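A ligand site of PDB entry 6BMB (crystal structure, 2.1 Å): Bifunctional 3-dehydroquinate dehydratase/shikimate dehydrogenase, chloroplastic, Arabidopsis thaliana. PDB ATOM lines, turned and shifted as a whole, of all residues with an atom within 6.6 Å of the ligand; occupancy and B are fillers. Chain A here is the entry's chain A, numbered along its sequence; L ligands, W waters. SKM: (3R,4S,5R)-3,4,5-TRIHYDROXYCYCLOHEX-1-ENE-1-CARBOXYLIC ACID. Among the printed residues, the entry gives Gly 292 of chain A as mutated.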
ATOM      1  N   ILE A 239     -17.583  -2.179  -2.956  1.00  0.00           N
ATOM      2  CA  ILE A 239     -17.771  -2.634  -4.316  1.00  0.00           C
ATOM      3  C   ILE A 239     -18.782  -3.787  -4.295  1.00  0.00           C
ATOM      4  O   ILE A 239     -18.480  -4.890  -3.819  1.00  0.00           O
ATOM      5  CB  ILE A 239     -16.437  -3.024  -4.979  1.00  0.00           C
ATOM      6  CG1 ILE A 239     -16.676  -3.730  -6.325  1.00  0.00           C
ATOM      7  CG2 ILE A 239     -15.527  -3.878  -4.035  1.00  0.00           C
ATOM      8  CD1 ILE A 239     -17.433  -2.904  -7.323  1.00  0.00           C
ATOM      9  N   VAL A 244     -16.227 -10.689  -6.550  1.00  0.00           N
ATOM     10  CA  VAL A 244     -15.811  -9.396  -6.044  1.00  0.00           C
ATOM     11  C   VAL A 244     -14.385  -9.484  -5.502  1.00  0.00           C
ATOM     12  O   VAL A 244     -13.715  -8.460  -5.349  1.00  0.00           O
ATOM     13  CB  VAL A 244     -16.799  -8.910  -4.962  1.00  0.00           C
ATOM     14  CG1 VAL A 244     -16.447  -9.438  -3.591  1.00  0.00           C
ATOM     15  CG2 VAL A 244     -16.898  -7.419  -4.974  1.00  0.00           C
ATOM     16  N   HIS A 246     -11.565 -10.170  -6.642  1.00  0.00           N
ATOM     17  CA  HIS A 246     -10.464  -9.623  -7.419  1.00  0.00           C
ATOM     18  C   HIS A 246     -10.378  -8.103  -7.305  1.00  0.00           C
ATOM     19  O   HIS A 246      -9.351  -7.548  -7.700  1.00  0.00           O
ATOM     20  CB  HIS A 246     -10.633  -9.980  -8.885  1.00  0.00           C
ATOM     21  CG  HIS A 246     -11.864  -9.366  -9.475  1.00  0.00           C
ATOM     22  ND1 HIS A 246     -13.119  -9.881  -9.251  1.00  0.00           N
ATOM     23  CD2 HIS A 246     -12.041  -8.226 -10.165  1.00  0.00           C
ATOM     24  CE1 HIS A 246     -14.016  -9.114  -9.829  1.00  0.00           C
ATOM     25  NE2 HIS A 246     -13.395  -8.089 -10.379  1.00  0.00           N
ATOM     26  N   SER A 247     -11.394  -7.424  -6.806  1.00  0.00           N
ATOM     27  CA  SER A 247     -11.474  -5.982  -6.991  1.00  0.00           C
ATOM     28  C   SER A 247     -10.396  -5.243  -6.221  1.00  0.00           C
ATOM     29  O   SER A 247     -10.102  -5.559  -5.057  1.00  0.00           O
ATOM     30  CB  SER A 247     -12.834  -5.431  -6.576  1.00  0.00           C
ATOM     31  OG  SER A 247     -12.781  -3.998  -6.541  1.00  0.00           O
ATOM     32  N   LYS A 248      -9.814  -4.253  -6.871  1.00  0.00           N
ATOM     33  CA  LYS A 248      -8.848  -3.361  -6.250  1.00  0.00           C
ATOM     34  C   LYS A 248      -9.451  -2.020  -5.900  1.00  0.00           C
ATOM     35  O   LYS A 248      -8.717  -1.125  -5.447  1.00  0.00           O
ATOM     36  CB  LYS A 248      -7.635  -3.202  -7.156  1.00  0.00           C
ATOM     37  CG  LYS A 248      -6.902  -4.499  -7.364  1.00  0.00           C
ATOM     38  CD  LYS A 248      -5.568  -4.327  -8.089  1.00  0.00           C
ATOM     39  CE  LYS A 248      -4.868  -5.687  -8.235  1.00  0.00           C
ATOM     40  NZ  LYS A 248      -3.602  -5.575  -8.999  1.00  0.00           N
ATOM     41  N   SER A 249     -10.758  -1.850  -6.060  1.00  0.00           N
ATOM     42  CA  SER A 249     -11.430  -0.673  -5.524  1.00  0.00           C
ATOM     43  C   SER A 249     -11.166  -0.458  -4.038  1.00  0.00           C
ATOM     44  O   SER A 249     -10.954   0.702  -3.625  1.00  0.00           O
ATOM     45  CB  SER A 249     -12.935  -0.736  -5.783  1.00  0.00           C
ATOM     46  OG  SER A 249     -13.265  -0.516  -7.149  1.00  0.00           O
ATOM     47  N   PRO A 250     -11.184  -1.476  -3.174  1.00  0.00           N
ATOM     48  CA  PRO A 250     -10.828  -1.204  -1.782  1.00  0.00           C
ATOM     49  C   PRO A 250      -9.400  -0.692  -1.620  1.00  0.00           C
ATOM     50  O   PRO A 250      -9.152   0.127  -0.737  1.00  0.00           O
ATOM     51  CB  PRO A 250     -11.052  -2.555  -1.096  1.00  0.00           C
ATOM     52  CG  PRO A 250     -12.124  -3.208  -1.982  1.00  0.00           C
ATOM     53  CD  PRO A 250     -11.673  -2.855  -3.349  1.00  0.00           C
ATOM     54  N   HIS A 253      -9.520   3.279  -2.998  1.00  0.00           N
ATOM     55  CA  HIS A 253     -10.371   4.241  -2.301  1.00  0.00           C
ATOM     56  C   HIS A 253      -9.939   4.428  -0.852  1.00  0.00           C
ATOM     57  O   HIS A 253      -9.886   5.556  -0.361  1.00  0.00           O
ATOM     58  CB  HIS A 253     -11.836   3.814  -2.428  1.00  0.00           C
ATOM     59  CG  HIS A 253     -12.335   3.862  -3.840  1.00  0.00           C
ATOM     60  ND1 HIS A 253     -12.218   5.005  -4.621  1.00  0.00           N
ATOM     61  CD2 HIS A 253     -12.863   2.909  -4.640  1.00  0.00           C
ATOM     62  CE1 HIS A 253     -12.690   4.747  -5.827  1.00  0.00           C
ATOM     63  NE2 HIS A 253     -13.090   3.490  -5.865  1.00  0.00           N
ATOM     64  N   TYR A 266     -13.741   1.460   2.753  1.00  0.00           N
ATOM     65  CA  TYR A 266     -14.242   0.804   1.547  1.00  0.00           C
ATOM     66  C   TYR A 266     -13.912  -0.693   1.621  1.00  0.00           C
ATOM     67  O   TYR A 266     -12.738  -1.056   1.769  1.00  0.00           O
ATOM     68  CB  TYR A 266     -13.612   1.448   0.316  1.00  0.00           C
ATOM     69  CG  TYR A 266     -14.255   1.108  -1.017  1.00  0.00           C
ATOM     70  CD1 TYR A 266     -14.083  -0.143  -1.592  1.00  0.00           C
ATOM     71  CD2 TYR A 266     -14.983   2.054  -1.709  1.00  0.00           C
ATOM     72  CE1 TYR A 266     -14.644  -0.456  -2.818  1.00  0.00           C
ATOM     73  CE2 TYR A 266     -15.552   1.759  -2.927  1.00  0.00           C
ATOM     74  CZ  TYR A 266     -15.382   0.504  -3.470  1.00  0.00           C
ATOM     75  OH  TYR A 266     -15.928   0.192  -4.679  1.00  0.00           O
ATOM     76  N   SER A 290     -19.897   1.200  -5.092  1.00  0.00           N
ATOM     77  CA  SER A 290     -19.626   0.955  -6.503  1.00  0.00           C
ATOM     78  C   SER A 290     -20.364  -0.314  -6.900  1.00  0.00           C
ATOM     79  O   SER A 290     -20.573  -1.209  -6.083  1.00  0.00           O
ATOM     80  CB  SER A 290     -18.111   0.825  -6.755  1.00  0.00           C
ATOM     81  OG  SER A 290     -17.359   1.814  -6.060  1.00  0.00           O
ATOM     82  N   CYS A 291     -20.759  -0.402  -8.181  1.00  0.00           N
ATOM     83  CA  CYS A 291     -21.545  -1.533  -8.681  1.00  0.00           C
ATOM     84  C   CYS A 291     -20.820  -2.207  -9.843  1.00  0.00           C
ATOM     85  O   CYS A 291     -20.629  -1.585 -10.894  1.00  0.00           O
ATOM     86  CB  CYS A 291     -22.927  -1.094  -9.150  1.00  0.00           C
ATOM     87  SG  CYS A 291     -23.995  -0.568  -7.825  1.00  0.00           S
ATOM     88  N   GLY A 292     -20.478  -3.482  -9.670  1.00  0.00           N
ATOM     89  CA  GLY A 292     -19.879  -4.265 -10.728  1.00  0.00           C
ATOM     90  C   GLY A 292     -20.803  -5.343 -11.250  1.00  0.00           C
ATOM     91  O   GLY A 292     -21.986  -5.414 -10.920  1.00  0.00           O
ATOM     92  N   ILE A 293     -20.228  -6.183 -12.111  1.00  0.00           N
ATOM     93  CA  ILE A 293     -20.911  -7.377 -12.604  1.00  0.00           C
ATOM     94  C   ILE A 293     -21.424  -8.185 -11.416  1.00  0.00           C
ATOM     95  O   ILE A 293     -20.699  -8.352 -10.437  1.00  0.00           O
ATOM     96  CB  ILE A 293     -19.959  -8.204 -13.492  1.00  0.00           C
ATOM     97  CG1 ILE A 293     -19.542  -7.383 -14.700  1.00  0.00           C
ATOM     98  CG2 ILE A 293     -20.624  -9.489 -13.970  1.00  0.00           C
ATOM     99  CD1 ILE A 293     -18.511  -8.046 -15.560  1.00  0.00           C
ATOM    100  N   LYS A 296     -24.997  -3.982 -12.332  1.00  0.00           N
ATOM    101  CA  LYS A 296     -25.058  -2.612 -12.831  1.00  0.00           C
ATOM    102  C   LYS A 296     -26.483  -2.245 -13.258  1.00  0.00           C
ATOM    103  O   LYS A 296     -26.977  -1.162 -12.899  1.00  0.00           O
ATOM    104  CB  LYS A 296     -24.086  -2.427 -14.002  1.00  0.00           C
ATOM    105  CG  LYS A 296     -22.599  -2.541 -13.644  1.00  0.00           C
ATOM    106  CD  LYS A 296     -21.747  -2.329 -14.892  1.00  0.00           C
ATOM    107  CE  LYS A 296     -20.273  -2.639 -14.667  1.00  0.00           C
ATOM    108  NZ  LYS A 296     -19.592  -1.582 -13.873  1.00  0.00           N
ATOM    109  N   ASN A 317     -23.204   2.323 -12.213  1.00  0.00           N
ATOM    110  CA  ASN A 317     -22.044   1.745 -11.530  1.00  0.00           C
ATOM    111  C   ASN A 317     -21.666   2.493 -10.251  1.00  0.00           C
ATOM    112  O   ASN A 317     -20.806   1.995  -9.516  1.00  0.00           O
ATOM    113  CB  ASN A 317     -20.836   1.684 -12.473  1.00  0.00           C
ATOM    114  CG  ASN A 317     -19.999   2.963 -12.476  1.00  0.00           C
ATOM    115  OD1 ASN A 317     -20.502   4.054 -12.232  1.00  0.00           O
ATOM    116  ND2 ASN A 317     -18.695   2.818 -12.748  1.00  0.00           N
ATOM    117  N   THR A 318     -22.290   3.630  -9.935  1.00  0.00           N
ATOM    118  CA  THR A 318     -22.033   4.320  -8.675  1.00  0.00           C
ATOM    119  C   THR A 318     -23.337   4.660  -7.971  1.00  0.00           C
ATOM    120  O   THR A 318     -24.198   5.338  -8.551  1.00  0.00           O
ATOM    121  CB  THR A 318     -21.204   5.591  -8.894  1.00  0.00           C
ATOM    122  OG1 THR A 318     -20.175   5.322  -9.836  1.00  0.00           O
ATOM    123  CG2 THR A 318     -20.573   6.051  -7.581  1.00  0.00           C
ATOM    124  N   THR A 333     -19.913   6.168 -14.101  1.00  0.00           N
ATOM    125  CA  THR A 333     -18.577   6.602 -14.439  1.00  0.00           C
ATOM    126  C   THR A 333     -17.850   5.619 -15.357  1.00  0.00           C
ATOM    127  O   THR A 333     -16.667   5.823 -15.640  1.00  0.00           O
ATOM    128  CB  THR A 333     -17.732   6.837 -13.175  1.00  0.00           C
ATOM    129  OG1 THR A 333     -17.433   5.573 -12.565  1.00  0.00           O
ATOM    130  CG2 THR A 333     -18.460   7.725 -12.168  1.00  0.00           C
ATOM    131  N   ASP A 334     -18.526   4.554 -15.815  1.00  0.00           N
ATOM    132  CA  ASP A 334     -17.890   3.656 -16.783  1.00  0.00           C
ATOM    133  C   ASP A 334     -17.716   4.346 -18.129  1.00  0.00           C
ATOM    134  O   ASP A 334     -16.714   4.098 -18.810  1.00  0.00           O
ATOM    135  CB  ASP A 334     -18.710   2.373 -16.977  1.00  0.00           C
ATOM    136  CG  ASP A 334     -18.530   1.369 -15.851  1.00  0.00           C
ATOM    137  OD1 ASP A 334     -17.383   1.092 -15.431  1.00  0.00           O
ATOM    138  OD2 ASP A 334     -19.561   0.854 -15.388  1.00  0.00           O
ATOM    139  N   ALA A 375     -21.310  -2.611 -18.415  1.00  0.00           N
ATOM    140  CA  ALA A 375     -20.081  -1.983 -18.913  1.00  0.00           C
ATOM    141  C   ALA A 375     -20.103  -1.848 -20.425  1.00  0.00           C
ATOM    142  O   ALA A 375     -19.532  -0.894 -20.969  1.00  0.00           O
ATOM    143  CB  ALA A 375     -18.862  -2.789 -18.464  1.00  0.00           C
ATOM    144  N   ALA A 459     -11.393  -4.003 -20.566  1.00  0.00           N
ATOM    145  CA  ALA A 459     -11.782  -3.489 -19.254  1.00  0.00           C
ATOM    146  C   ALA A 459     -11.262  -4.342 -18.104  1.00  0.00           C
ATOM    147  O   ALA A 459     -11.133  -3.838 -16.979  1.00  0.00           O
ATOM    148  CB  ALA A 459     -13.305  -3.380 -19.157  1.00  0.00           C
ATOM    149  N   TYR A 461      -8.848  -5.648 -15.623  1.00  0.00           N
ATOM    150  CA  TYR A 461      -7.568  -5.134 -15.139  1.00  0.00           C
ATOM    151  C   TYR A 461      -6.870  -6.116 -14.195  1.00  0.00           C
ATOM    152  O   TYR A 461      -5.785  -5.807 -13.677  1.00  0.00           O
ATOM    153  CB  TYR A 461      -7.758  -3.769 -14.461  1.00  0.00           C
ATOM    154  CG  TYR A 461      -8.584  -3.799 -13.202  1.00  0.00           C
ATOM    155  CD1 TYR A 461      -9.978  -3.786 -13.272  1.00  0.00           C
ATOM    156  CD2 TYR A 461      -7.980  -3.848 -11.959  1.00  0.00           C
ATOM    157  CE1 TYR A 461     -10.738  -3.830 -12.106  1.00  0.00           C
ATOM    158  CE2 TYR A 461      -8.729  -3.885 -10.799  1.00  0.00           C
ATOM    159  CZ  TYR A 461     -10.095  -3.880 -10.876  1.00  0.00           C
ATOM    160  OH  TYR A 461     -10.830  -3.936  -9.711  1.00  0.00           O
ATOM    161  N   MET A 485      -8.790   2.481 -17.668  1.00  0.00           N
ATOM    162  CA  MET A 485     -10.203   2.741 -17.424  1.00  0.00           C
ATOM    163  C   MET A 485     -10.513   2.682 -15.941  1.00  0.00           C
ATOM    164  O   MET A 485     -11.318   3.472 -15.429  1.00  0.00           O
ATOM    165  CB  MET A 485     -11.043   1.729 -18.214  1.00  0.00           C
ATOM    166  CG  MET A 485     -12.560   1.663 -17.940  1.00  0.00           C
ATOM    167  SD  MET A 485     -13.173   1.152 -16.306  1.00  0.00           S
ATOM    168  CE  MET A 485     -12.911  -0.602 -16.330  1.00  0.00           C
ATOM    169  N   PHE A 486      -9.887   1.737 -15.219  1.00  0.00           N
ATOM    170  CA  PHE A 486     -10.256   1.539 -13.828  1.00  0.00           C
ATOM    171  C   PHE A 486      -9.906   2.756 -12.984  1.00  0.00           C
ATOM    172  O   PHE A 486     -10.716   3.211 -12.173  1.00  0.00           O
ATOM    173  CB  PHE A 486      -9.575   0.297 -13.261  1.00  0.00           C
ATOM    174  CG  PHE A 486      -9.814   0.124 -11.796  1.00  0.00           C
ATOM    175  CD1 PHE A 486     -11.040  -0.322 -11.340  1.00  0.00           C
ATOM    176  CD2 PHE A 486      -8.828   0.424 -10.879  1.00  0.00           C
ATOM    177  CE1 PHE A 486     -11.265  -0.485  -9.994  1.00  0.00           C
ATOM    178  CE2 PHE A 486      -9.044   0.263  -9.530  1.00  0.00           C
ATOM    179  CZ  PHE A 486     -10.275  -0.194  -9.081  1.00  0.00           C
ATOM    180  N   GLN A 489     -12.385   5.734 -13.898  1.00  0.00           N
ATOM    181  CA  GLN A 489     -13.722   5.648 -13.327  1.00  0.00           C
ATOM    182  C   GLN A 489     -13.688   5.713 -11.809  1.00  0.00           C
ATOM    183  O   GLN A 489     -14.705   6.041 -11.195  1.00  0.00           O
ATOM    184  CB  GLN A 489     -14.447   4.369 -13.772  1.00  0.00           C
ATOM    185  CG  GLN A 489     -13.878   3.058 -13.215  1.00  0.00           C
ATOM    186  CD  GLN A 489     -14.357   2.747 -11.810  1.00  0.00           C
ATOM    187  OE1 GLN A 489     -15.489   3.054 -11.438  1.00  0.00           O
ATOM    188  NE2 GLN A 489     -13.482   2.138 -11.014  1.00  0.00           N
ATOM    189  N   GLN A 493     -15.584   8.264  -9.000  1.00  0.00           N
ATOM    190  CA  GLN A 493     -16.438   7.802  -7.910  1.00  0.00           C
ATOM    191  C   GLN A 493     -16.053   8.436  -6.574  1.00  0.00           C
ATOM    192  O   GLN A 493     -16.929   8.737  -5.747  1.00  0.00           O
ATOM    193  CB  GLN A 493     -16.400   6.271  -7.808  1.00  0.00           C
ATOM    194  CG  GLN A 493     -16.964   5.549  -9.009  1.00  0.00           C
ATOM    195  CD  GLN A 493     -17.071   4.034  -8.787  1.00  0.00           C
ATOM    196  OE1 GLN A 493     -16.276   3.451  -8.057  1.00  0.00           O
ATOM    197  NE2 GLN A 493     -18.072   3.425  -9.395  1.00  0.00           N
HETATM  198  O12 SKM L   1     -17.468   0.053 -12.890  1.00  0.00           O
HETATM  199  C8  SKM L   1     -16.339  -0.378 -12.172  1.00  0.00           C
HETATM  200  C6  SKM L   1     -16.772  -0.575 -10.682  1.00  0.00           C
HETATM  201  O7  SKM L   1     -17.292   0.636 -10.237  1.00  0.00           O
HETATM  202  C5  SKM L   1     -15.552  -1.023  -9.853  1.00  0.00           C
HETATM  203  C4  SKM L   1     -14.909  -2.198 -10.454  1.00  0.00           C
HETATM  204  C1  SKM L   1     -13.988  -2.985  -9.576  1.00  0.00           C
HETATM  205  O2  SKM L   1     -13.379  -3.921 -10.140  1.00  0.00           O
HETATM  206  O3  SKM L   1     -13.886  -2.662  -8.381  1.00  0.00           O
HETATM  207  C10 SKM L   1     -14.845  -2.378 -11.760  1.00  0.00           C
HETATM  208  C9  SKM L   1     -15.771  -1.719 -12.731  1.00  0.00           C
HETATM  209  O11 SKM L   1     -16.874  -2.525 -13.053  1.00  0.00           O
HETATM  210  O   HOH W   1     -14.071  -5.827 -11.858  1.00  0.00           O
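Water W1 lies within hydrogen-bond range of an oxygen (O2) of the ligand and a ring nitrogen (NE2) of His 246.
The side-chain hydroxyl of Tyr 461 is in hydrogen-bond range of the backbone NH of Lys 248.
The side-chain carboxylate (OD2) of Asp 334 lies within salt-bridge range of the side-chain amino group (NZ) of Lys 296, at 2.9 Å.
O of Cys 291 sits at hydrogen-bond distance from NZ of Lys 296 (3.2 Å).
The side-chain amide oxygen of Gln 493 is in hydrogen-bond range of the side-chain hydroxyl of Ser 290 (2.8 Å).
The side-chain amide nitrogen of Asn 317 is in hydrogen-bond range of the side-chain amide oxygen of Gln 489 (3.5 Å).
O of Asn 317 lies within hydrogen-bond range of N of Cys 291 (2.7 Å).
O of Phe 486 is in hydrogen-bond range of NE2 of Gln 489 (3.2 Å).
OG of Ser 290 sits at hydrogen-bond distance from OH of Tyr 266 (2.6 Å).
The side-chain hydroxyl (OG) of Ser 247 sits at hydrogen-bond distance from an oxygen (O3) of the ligand, 2.5 Å away.
An oxygen (O3) of the ligand lies within hydrogen-bond range of the side-chain hydroxyl (OG) of Ser 249 (2.6 Å).
An oxygen (O2) of the ligand lies within hydrogen-bond range of the side-chain hydroxyl of Tyr 461 (2.6 Å).
O12 of the ligand is in hydrogen-bond range of OD1 of Asp 334 (2.7 Å).
The side-chain amino group of Lys 296 sits at hydrogen-bond distance from an oxygen (O12) of the ligand, at 2.9 Å.
NE2 of Gln 493 lies within hydrogen-bond range of O7 of the ligand (3.0 Å).
O12 of the ligand lies within hydrogen-bond range of ND2 of Asn 317 (3.0 Å).
The side-chain amide oxygen (OE1) of Gln 489 is in hydrogen-bond range of an oxygen (O7) of the ligand (3.2 Å).
Ile 239 touches the ligand.
Ser 290 touches the ligand (CB to O7, 3.6 Å).
Cys 291 touches the ligand (O to C6, 3.99 Å).
CE1 of Phe 486 touches C1 of the ligand, 3.7 Å away.
Hydrophobic or aromatic side chains that line the ligand: Ile 239, Tyr 461 and Phe 486.
12 residues have an atom within 4 Å of the ligand: Ile 239, Ser 247, Ser 249, Ser 290, Cys 291, Lys 296, Asn 317, Asp 334, Tyr 461, Phe 486, Gln 489 and Gln 493.
The nearest printed residue that does not touch the ligand is His 246 (4.2 Å).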
